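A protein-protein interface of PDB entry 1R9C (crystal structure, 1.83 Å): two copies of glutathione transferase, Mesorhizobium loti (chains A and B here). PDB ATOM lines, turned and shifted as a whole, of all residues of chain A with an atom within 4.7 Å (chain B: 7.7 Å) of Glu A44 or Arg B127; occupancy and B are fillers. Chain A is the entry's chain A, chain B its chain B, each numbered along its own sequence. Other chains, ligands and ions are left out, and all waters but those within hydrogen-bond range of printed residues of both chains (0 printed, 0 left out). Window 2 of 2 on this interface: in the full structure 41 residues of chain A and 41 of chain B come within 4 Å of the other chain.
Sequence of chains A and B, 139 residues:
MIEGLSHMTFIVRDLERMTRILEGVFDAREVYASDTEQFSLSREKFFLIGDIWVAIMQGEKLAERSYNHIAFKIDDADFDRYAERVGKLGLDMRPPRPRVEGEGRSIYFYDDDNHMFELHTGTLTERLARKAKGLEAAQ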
ATOM      1  N   LEU A  15     -22.308 -14.271  10.502  1.00  0.00           N
ATOM      2  CA  LEU A  15     -22.122 -15.209  11.605  1.00  0.00           C
ATOM      3  C   LEU A  15     -22.637 -14.734  12.962  1.00  0.00           C
ATOM      4  O   LEU A  15     -23.046 -15.551  13.824  1.00  0.00           O
ATOM      5  CB  LEU A  15     -20.629 -15.494  11.783  1.00  0.00           C
ATOM      6  CG  LEU A  15     -19.880 -16.624  11.094  1.00  0.00           C
ATOM      7  CD1 LEU A  15     -18.542 -16.882  11.806  1.00  0.00           C
ATOM      8  CD2 LEU A  15     -20.690 -17.887  11.056  1.00  0.00           C
ATOM      9  N   TYR A  32     -17.348 -23.571  19.785  1.00  0.00           N
ATOM     10  CA  TYR A  32     -16.125 -23.340  19.010  1.00  0.00           C
ATOM     11  C   TYR A  32     -16.306 -22.148  18.100  1.00  0.00           C
ATOM     12  O   TYR A  32     -17.385 -21.970  17.523  1.00  0.00           O
ATOM     13  CB  TYR A  32     -15.791 -24.560  18.142  1.00  0.00           C
ATOM     14  CG  TYR A  32     -14.655 -24.337  17.134  1.00  0.00           C
ATOM     15  CD1 TYR A  32     -13.309 -24.420  17.529  1.00  0.00           C
ATOM     16  CD2 TYR A  32     -14.935 -24.042  15.790  1.00  0.00           C
ATOM     17  CE1 TYR A  32     -12.262 -24.225  16.597  1.00  0.00           C
ATOM     18  CE2 TYR A  32     -13.888 -23.849  14.853  1.00  0.00           C
ATOM     19  CZ  TYR A  32     -12.579 -23.943  15.261  1.00  0.00           C
ATOM     20  OH  TYR A  32     -11.584 -23.743  14.328  1.00  0.00           O
ATOM     21  N   ALA A  33     -15.235 -21.357  17.969  1.00  0.00           N
ATOM     22  CA  ALA A  33     -15.154 -20.294  16.969  1.00  0.00           C
ATOM     23  C   ALA A  33     -13.754 -20.265  16.365  1.00  0.00           C
ATOM     24  O   ALA A  33     -12.753 -20.141  17.081  1.00  0.00           O
ATOM     25  CB  ALA A  33     -15.525 -18.911  17.578  1.00  0.00           C
ATOM     26  N   SER A  34     -13.684 -20.374  15.041  1.00  0.00           N
ATOM     27  CA  SER A  34     -12.409 -20.305  14.340  1.00  0.00           C
ATOM     28  C   SER A  34     -11.708 -18.952  14.521  1.00  0.00           C
ATOM     29  O   SER A  34     -10.499 -18.863  14.366  1.00  0.00           O
ATOM     30  CB  SER A  34     -12.571 -20.663  12.862  1.00  0.00           C
ATOM     31  OG  SER A  34     -13.281 -19.656  12.184  1.00  0.00           O
ATOM     32  N   SER A  42     -11.089 -18.152   6.773  1.00  0.00           N
ATOM     33  CA  SER A  42     -12.465 -18.596   6.787  1.00  0.00           C
ATOM     34  C   SER A  42     -12.977 -18.542   8.229  1.00  0.00           C
ATOM     35  O   SER A  42     -12.203 -18.730   9.183  1.00  0.00           O
ATOM     36  CB  SER A  42     -12.541 -20.005   6.215  1.00  0.00           C
ATOM     37  OG  SER A  42     -11.936 -20.925   7.095  1.00  0.00           O
ATOM     38  N   ARG A  43     -14.265 -18.251   8.374  1.00  0.00           N
ATOM     39  CA  ARG A  43     -14.885 -18.094   9.685  1.00  0.00           C
ATOM     40  C   ARG A  43     -16.012 -19.095   9.910  1.00  0.00           C
ATOM     41  O   ARG A  43     -16.971 -19.137   9.158  1.00  0.00           O
ATOM     42  CB  ARG A  43     -15.404 -16.663   9.842  1.00  0.00           C
ATOM     43  CG  ARG A  43     -14.323 -15.628   9.514  1.00  0.00           C
ATOM     44  CD  ARG A  43     -14.632 -14.220   9.936  1.00  0.00           C
ATOM     45  NE  ARG A  43     -15.205 -14.134  11.280  1.00  0.00           N
ATOM     46  CZ  ARG A  43     -16.445 -13.696  11.548  1.00  0.00           C
ATOM     47  NH1 ARG A  43     -17.270 -13.317  10.569  1.00  0.00           N
ATOM     48  NH2 ARG A  43     -16.854 -13.637  12.806  1.00  0.00           N
ATOM     49  N   GLU A  44     -15.879 -19.901  10.958  1.00  0.00           N
ATOM     50  CA  GLU A  44     -16.894 -20.892  11.280  1.00  0.00           C
ATOM     51  C   GLU A  44     -17.121 -20.923  12.790  1.00  0.00           C
ATOM     52  O   GLU A  44     -16.240 -20.511  13.564  1.00  0.00           O
ATOM     53  CB  GLU A  44     -16.505 -22.279  10.729  1.00  0.00           C
ATOM     54  CG  GLU A  44     -15.374 -22.968  11.463  1.00  0.00           C
ATOM     55  CD  GLU A  44     -14.834 -24.189  10.725  1.00  0.00           C
ATOM     56  OE1 GLU A  44     -15.619 -24.922  10.083  1.00  0.00           O
ATOM     57  OE2 GLU A  44     -13.610 -24.413  10.804  1.00  0.00           O
ATOM     58  N   LYS A  45     -18.310 -21.373  13.195  1.00  0.00           N
ATOM     59  CA  LYS A  45     -18.616 -21.645  14.587  1.00  0.00           C
ATOM     60  C   LYS A  45     -19.357 -22.952  14.686  1.00  0.00           C
ATOM     61  O   LYS A  45     -20.091 -23.319  13.759  1.00  0.00           O
ATOM     62  CB  LYS A  45     -19.547 -20.561  15.144  1.00  0.00           C
ATOM     63  CG  LYS A  45     -18.904 -19.180  15.326  1.00  0.00           C
ATOM     64  CD  LYS A  45     -19.902 -18.268  15.948  1.00  0.00           C
ATOM     65  CE  LYS A  45     -19.297 -16.980  16.445  1.00  0.00           C
ATOM     66  NZ  LYS A  45     -20.259 -16.409  17.447  1.00  0.00           N
ATOM     67  N   PHE A  46     -19.173 -23.651  15.811  1.00  0.00           N
ATOM     68  CA  PHE A  46     -19.914 -24.877  16.112  1.00  0.00           C
ATOM     69  C   PHE A  46     -20.808 -24.603  17.333  1.00  0.00           C
ATOM     70  O   PHE A  46     -20.375 -23.937  18.316  1.00  0.00           O
ATOM     71  CB  PHE A  46     -18.978 -26.019  16.495  1.00  0.00           C
ATOM     72  CG  PHE A  46     -18.021 -26.455  15.412  1.00  0.00           C
ATOM     73  CD1 PHE A  46     -16.873 -27.149  15.755  1.00  0.00           C
ATOM     74  CD2 PHE A  46     -18.288 -26.209  14.061  1.00  0.00           C
ATOM     75  CE1 PHE A  46     -15.977 -27.599  14.778  1.00  0.00           C
ATOM     76  CE2 PHE A  46     -17.402 -26.624  13.079  1.00  0.00           C
ATOM     77  CZ  PHE A  46     -16.245 -27.337  13.434  1.00  0.00           C
ATOM     78  N   TRP A  53     -25.106 -31.233  16.891  1.00  0.00           N
ATOM     79  CA  TRP A  53     -24.030 -30.377  16.402  1.00  0.00           C
ATOM     80  C   TRP A  53     -24.516 -29.599  15.186  1.00  0.00           C
ATOM     81  O   TRP A  53     -24.890 -30.206  14.168  1.00  0.00           O
ATOM     82  CB  TRP A  53     -22.879 -31.290  16.024  1.00  0.00           C
ATOM     83  CG  TRP A  53     -21.607 -30.693  15.497  1.00  0.00           C
ATOM     84  CD1 TRP A  53     -21.237 -29.378  15.424  1.00  0.00           C
ATOM     85  CD2 TRP A  53     -20.508 -31.445  14.986  1.00  0.00           C
ATOM     86  NE1 TRP A  53     -19.980 -29.274  14.876  1.00  0.00           N
ATOM     87  CE2 TRP A  53     -19.501 -30.526  14.613  1.00  0.00           C
ATOM     88  CE3 TRP A  53     -20.270 -32.814  14.808  1.00  0.00           C
ATOM     89  CZ2 TRP A  53     -18.269 -30.934  14.077  1.00  0.00           C
ATOM     90  CZ3 TRP A  53     -19.037 -33.221  14.288  1.00  0.00           C
ATOM     91  CH2 TRP A  53     -18.064 -32.284  13.924  1.00  0.00           C
ATOM     92  N   ILE A  56     -21.909 -23.467  11.535  1.00  0.00           N
ATOM     93  CA  ILE A  56     -22.144 -22.388  10.604  1.00  0.00           C
ATOM     94  C   ILE A  56     -20.834 -21.859  10.060  1.00  0.00           C
ATOM     95  O   ILE A  56     -19.820 -21.798  10.787  1.00  0.00           O
ATOM     96  CB  ILE A  56     -23.030 -21.259  11.216  1.00  0.00           C
ATOM     97  CG1 ILE A  56     -22.385 -20.610  12.465  1.00  0.00           C
ATOM     98  CG2 ILE A  56     -24.439 -21.817  11.559  1.00  0.00           C
ATOM     99  CD1 ILE A  56     -23.186 -19.452  13.019  1.00  0.00           C
ATOM    100  N   MET A  57     -20.859 -21.484   8.777  1.00  0.00           N
ATOM    101  CA  MET A  57     -19.699 -20.890   8.122  1.00  0.00           C
ATOM    102  C   MET A  57     -20.141 -19.665   7.347  1.00  0.00           C
ATOM    103  O   MET A  57     -21.223 -19.653   6.795  1.00  0.00           O
ATOM    104  CB  MET A  57     -18.982 -21.890   7.198  1.00  0.00           C
ATOM    105  CG  MET A  57     -18.936 -23.360   7.698  1.00  0.00           C
ATOM    106  SD  MET A  57     -18.303 -24.528   6.415  1.00  0.00           S
ATOM    107  CE  MET A  57     -17.202 -23.352   5.410  1.00  0.00           C
ATOM    108  N   HIS B  69     -25.195 -28.609   4.138  1.00  0.00           N
ATOM    109  CA  HIS B  69     -25.174 -30.081   4.096  1.00  0.00           C
ATOM    110  C   HIS B  69     -25.659 -30.700   5.389  1.00  0.00           C
ATOM    111  O   HIS B  69     -25.605 -30.072   6.468  1.00  0.00           O
ATOM    112  CB  HIS B  69     -23.778 -30.671   3.672  1.00  0.00           C
ATOM    113  CG  HIS B  69     -22.652 -30.455   4.654  1.00  0.00           C
ATOM    114  ND1 HIS B  69     -21.807 -29.376   4.578  1.00  0.00           N
ATOM    115  CD2 HIS B  69     -22.156 -31.247   5.644  1.00  0.00           C
ATOM    116  CE1 HIS B  69     -20.877 -29.476   5.518  1.00  0.00           C
ATOM    117  NE2 HIS B  69     -21.063 -30.601   6.185  1.00  0.00           N
ATOM    118  N   GLY B 104     -10.452 -39.193  10.662  1.00  0.00           N
ATOM    119  CA  GLY B 104     -11.504 -38.186  10.748  1.00  0.00           C
ATOM    120  C   GLY B 104     -11.952 -37.891   9.317  1.00  0.00           C
ATOM    121  O   GLY B 104     -11.700 -36.808   8.794  1.00  0.00           O
ATOM    122  N   SER B 106     -14.449 -38.037   5.575  1.00  0.00           N
ATOM    123  CA  SER B 106     -15.811 -37.775   5.056  1.00  0.00           C
ATOM    124  C   SER B 106     -16.007 -38.220   3.608  1.00  0.00           C
ATOM    125  O   SER B 106     -15.077 -38.184   2.814  1.00  0.00           O
ATOM    126  CB  SER B 106     -16.166 -36.288   5.122  1.00  0.00           C
ATOM    127  OG  SER B 106     -16.212 -35.801   6.448  1.00  0.00           O
ATOM    128  N   TYR B 108     -18.548 -36.888   0.634  1.00  0.00           N
ATOM    129  CA  TYR B 108     -19.520 -35.874   0.257  1.00  0.00           C
ATOM    130  C   TYR B 108     -20.144 -36.251  -1.070  1.00  0.00           C
ATOM    131  O   TYR B 108     -19.434 -36.692  -1.961  1.00  0.00           O
ATOM    132  CB  TYR B 108     -18.842 -34.499   0.105  1.00  0.00           C
ATOM    133  CG  TYR B 108     -18.233 -33.938   1.389  1.00  0.00           C
ATOM    134  CD1 TYR B 108     -16.886 -34.134   1.658  1.00  0.00           C
ATOM    135  CD2 TYR B 108     -18.996 -33.203   2.310  1.00  0.00           C
ATOM    136  CE1 TYR B 108     -16.301 -33.628   2.798  1.00  0.00           C
ATOM    137  CE2 TYR B 108     -18.407 -32.690   3.489  1.00  0.00           C
ATOM    138  CZ  TYR B 108     -17.047 -32.928   3.712  1.00  0.00           C
ATOM    139  OH  TYR B 108     -16.376 -32.464   4.836  1.00  0.00           O
ATOM    140  N   GLU B 118     -23.319 -35.770   3.598  1.00  0.00           N
ATOM    141  CA  GLU B 118     -21.980 -36.125   4.035  1.00  0.00           C
ATOM    142  C   GLU B 118     -22.098 -37.363   4.939  1.00  0.00           C
ATOM    143  O   GLU B 118     -23.048 -37.487   5.720  1.00  0.00           O
ATOM    144  CB  GLU B 118     -21.349 -34.944   4.788  1.00  0.00           C
ATOM    145  CG  GLU B 118     -20.074 -35.286   5.557  1.00  0.00           C
ATOM    146  CD  GLU B 118     -19.454 -34.138   6.356  1.00  0.00           C
ATOM    147  OE1 GLU B 118     -20.020 -33.007   6.495  1.00  0.00           O
ATOM    148  OE2 GLU B 118     -18.326 -34.396   6.877  1.00  0.00           O
ATOM    149  N   HIS B 120     -19.661 -39.117   7.727  1.00  0.00           N
ATOM    150  CA  HIS B 120     -18.513 -38.619   8.459  1.00  0.00           C
ATOM    151  C   HIS B 120     -18.148 -39.630   9.549  1.00  0.00           C
ATOM    152  O   HIS B 120     -19.029 -40.085  10.278  1.00  0.00           O
ATOM    153  CB  HIS B 120     -18.854 -37.230   9.052  1.00  0.00           C
ATOM    154  CG  HIS B 120     -17.740 -36.609   9.840  1.00  0.00           C
ATOM    155  ND1 HIS B 120     -16.449 -36.506   9.357  1.00  0.00           N
ATOM    156  CD2 HIS B 120     -17.717 -36.091  11.092  1.00  0.00           C
ATOM    157  CE1 HIS B 120     -15.687 -35.924  10.269  1.00  0.00           C
ATOM    158  NE2 HIS B 120     -16.438 -35.650  11.324  1.00  0.00           N
ATOM    159  N   GLY B 122     -15.809 -39.053  12.109  1.00  0.00           N
ATOM    160  CA  GLY B 122     -15.307 -38.413  13.333  1.00  0.00           C
ATOM    161  C   GLY B 122     -16.385 -37.863  14.271  1.00  0.00           C
ATOM    162  O   GLY B 122     -17.570 -37.915  13.965  1.00  0.00           O
ATOM    163  N   THR B 123     -15.982 -37.364  15.440  1.00  0.00           N
ATOM    164  CA  THR B 123     -16.943 -36.805  16.388  1.00  0.00           C
ATOM    165  C   THR B 123     -16.611 -35.347  16.635  1.00  0.00           C
ATOM    166  O   THR B 123     -15.527 -34.873  16.291  1.00  0.00           O
ATOM    167  CB  THR B 123     -16.930 -37.589  17.735  1.00  0.00           C
ATOM    168  OG1 THR B 123     -15.613 -37.562  18.282  1.00  0.00           O
ATOM    169  CG2 THR B 123     -17.184 -39.083  17.504  1.00  0.00           C
ATOM    170  N   LEU B 124     -17.544 -34.646  17.261  1.00  0.00           N
ATOM    171  CA  LEU B 124     -17.330 -33.262  17.650  1.00  0.00           C
ATOM    172  C   LEU B 124     -16.154 -33.146  18.576  1.00  0.00           C
ATOM    173  O   LEU B 124     -15.279 -32.313  18.347  1.00  0.00           O
ATOM    174  CB  LEU B 124     -18.596 -32.696  18.306  1.00  0.00           C
ATOM    175  CG  LEU B 124     -18.539 -31.290  18.911  1.00  0.00           C
ATOM    176  CD1 LEU B 124     -18.094 -30.224  17.895  1.00  0.00           C
ATOM    177  CD2 LEU B 124     -19.892 -30.953  19.524  1.00  0.00           C
ATOM    178  N   THR B 125     -16.137 -33.986  19.618  1.00  0.00           N
ATOM    179  CA  THR B 125     -15.037 -34.034  20.583  1.00  0.00           C
ATOM    180  C   THR B 125     -13.678 -34.137  19.888  1.00  0.00           C
ATOM    181  O   THR B 125     -12.766 -33.367  20.193  1.00  0.00           O
ATOM    182  CB  THR B 125     -15.231 -35.206  21.586  1.00  0.00           C
ATOM    183  OG1 THR B 125     -16.448 -35.023  22.318  1.00  0.00           O
ATOM    184  CG2 THR B 125     -14.175 -35.172  22.673  1.00  0.00           C
ATOM    185  N   GLU B 126     -13.553 -35.084  18.960  1.00  0.00           N
ATOM    186  CA  GLU B 126     -12.303 -35.295  18.226  1.00  0.00           C
ATOM    187  C   GLU B 126     -11.944 -34.038  17.451  1.00  0.00           C
ATOM    188  O   GLU B 126     -10.799 -33.586  17.493  1.00  0.00           O
ATOM    189  CB  GLU B 126     -12.427 -36.472  17.250  1.00  0.00           C
ATOM    190  CG  GLU B 126     -12.149 -37.836  17.855  1.00  0.00           C
ATOM    191  CD  GLU B 126     -12.815 -38.965  17.083  1.00  0.00           C
ATOM    192  OE1 GLU B 126     -12.919 -40.069  17.640  1.00  0.00           O
ATOM    193  OE2 GLU B 126     -13.232 -38.762  15.920  1.00  0.00           O
ATOM    194  N   ARG B 127     -12.936 -33.478  16.761  1.00  0.00           N
ATOM    195  CA  ARG B 127     -12.756 -32.274  15.957  1.00  0.00           C
ATOM    196  C   ARG B 127     -12.301 -31.087  16.819  1.00  0.00           C
ATOM    197  O   ARG B 127     -11.424 -30.317  16.404  1.00  0.00           O
ATOM    198  CB  ARG B 127     -14.042 -31.961  15.176  1.00  0.00           C
ATOM    199  CG  ARG B 127     -13.985 -30.711  14.330  1.00  0.00           C
ATOM    200  CD  ARG B 127     -14.254 -30.930  12.856  1.00  0.00           C
ATOM    201  NE  ARG B 127     -13.587 -29.887  12.073  1.00  0.00           N
ATOM    202  CZ  ARG B 127     -14.106 -29.290  11.005  1.00  0.00           C
ATOM    203  NH1 ARG B 127     -15.313 -29.635  10.566  1.00  0.00           N
ATOM    204  NH2 ARG B 127     -13.408 -28.347  10.376  1.00  0.00           N
ATOM    205  N   LEU B 128     -12.859 -30.970  18.026  1.00  0.00           N
ATOM    206  CA  LEU B 128     -12.454 -29.925  18.965  1.00  0.00           C
ATOM    207  C   LEU B 128     -11.000 -30.054  19.425  1.00  0.00           C
ATOM    208  O   LEU B 128     -10.489 -29.161  20.106  1.00  0.00           O
ATOM    209  CB  LEU B 128     -13.386 -29.864  20.185  1.00  0.00           C
ATOM    210  CG  LEU B 128     -14.827 -29.379  19.963  1.00  0.00           C
ATOM    211  CD1 LEU B 128     -15.659 -29.535  21.233  1.00  0.00           C
ATOM    212  CD2 LEU B 128     -14.885 -27.948  19.426  1.00  0.00           C
ATOM    213  N   ALA B 129     -10.334 -31.147  19.048  1.00  0.00           N
ATOM    214  CA  ALA B 129      -8.917 -31.325  19.386  1.00  0.00           C
ATOM    215  C   ALA B 129      -7.987 -30.817  18.274  1.00  0.00           C
ATOM    216  O   ALA B 129      -7.430 -29.723  18.332  1.00  0.00           O
ATOM    217  CB  ALA B 129      -8.624 -32.778  19.728  1.00  0.00           C
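The guanidinium group (NH2) of Arg B127 is in salt-bridge range of the side-chain carboxylate (OE2) of Glu A44 (3.96 Å).
Among the printed residues, pairs that only touch across the chains: Tyr A32 with Leu B128, Phe A46 with Leu B124, Phe A46 with Arg B127, Trp A53 with Thr B123 and Trp A53 with Leu B124.
The backbone carbonyl oxygen (O) of Tyr A32 sits at hydrogen-bond distance from the backbone NH (N) of Phe A46 (3.0 Å).
The side-chain hydroxyl of Ser A34 is in hydrogen-bond range of the backbone NH of Glu A44 (2.9 Å).
The backbone NH (N) of Thr B123 lies within hydrogen-bond range of the side-chain carboxylate (OE2) of Glu B126, at 3.1 Å.
Of the 12 printed residues of chain A, 4 touch a printed residue of chain B.
Hydrophobic or aromatic side chains of chain A that line the printed part of chain B: Tyr A32, Phe A46 and Trp A53.
Printed residues of chain B that touch a printed residue of chain A: Thr B123, Leu B124, Arg B127 and Leu B128.
Hydrophobic or aromatic side chains of chain B within 4 Å of the printed part of chain A: Leu B124 and Leu B128.
Along chain B the printed residues that touch a printed residue of chain A span positions 123 to 128.
Among the printed residues, Asp or Glu carboxylates within 4 Å of a Lys or Arg side-chain nitrogen of the other chain: Glu A44 with Arg B127.
No position is printed for both chains.
Printed residues of chain B within 4 Å of Glu A44: Arg B127.
Of chain A, only Glu A44 and Phe A46 come within 4 Å of Arg B127.
Of the printed residues of chain B, Tyr A32 touches Leu B128.
Of the printed residues of chain B, Phe A46 touches Leu B124 and Arg B127.
Printed residues of chain B within 4 Å of Trp A53: Thr B123 and Leu B124.
Of the printed residues of chain A, Thr B123 touches Trp A53.
Printed residues of chain A within 4 Å of Leu B124: Phe A46 and Trp A53.
Glu B126 touches none of the printed residues of chain A.
The nearest residue of chain A that does not touch Arg B127 is Trp A53 (4.2 Å).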
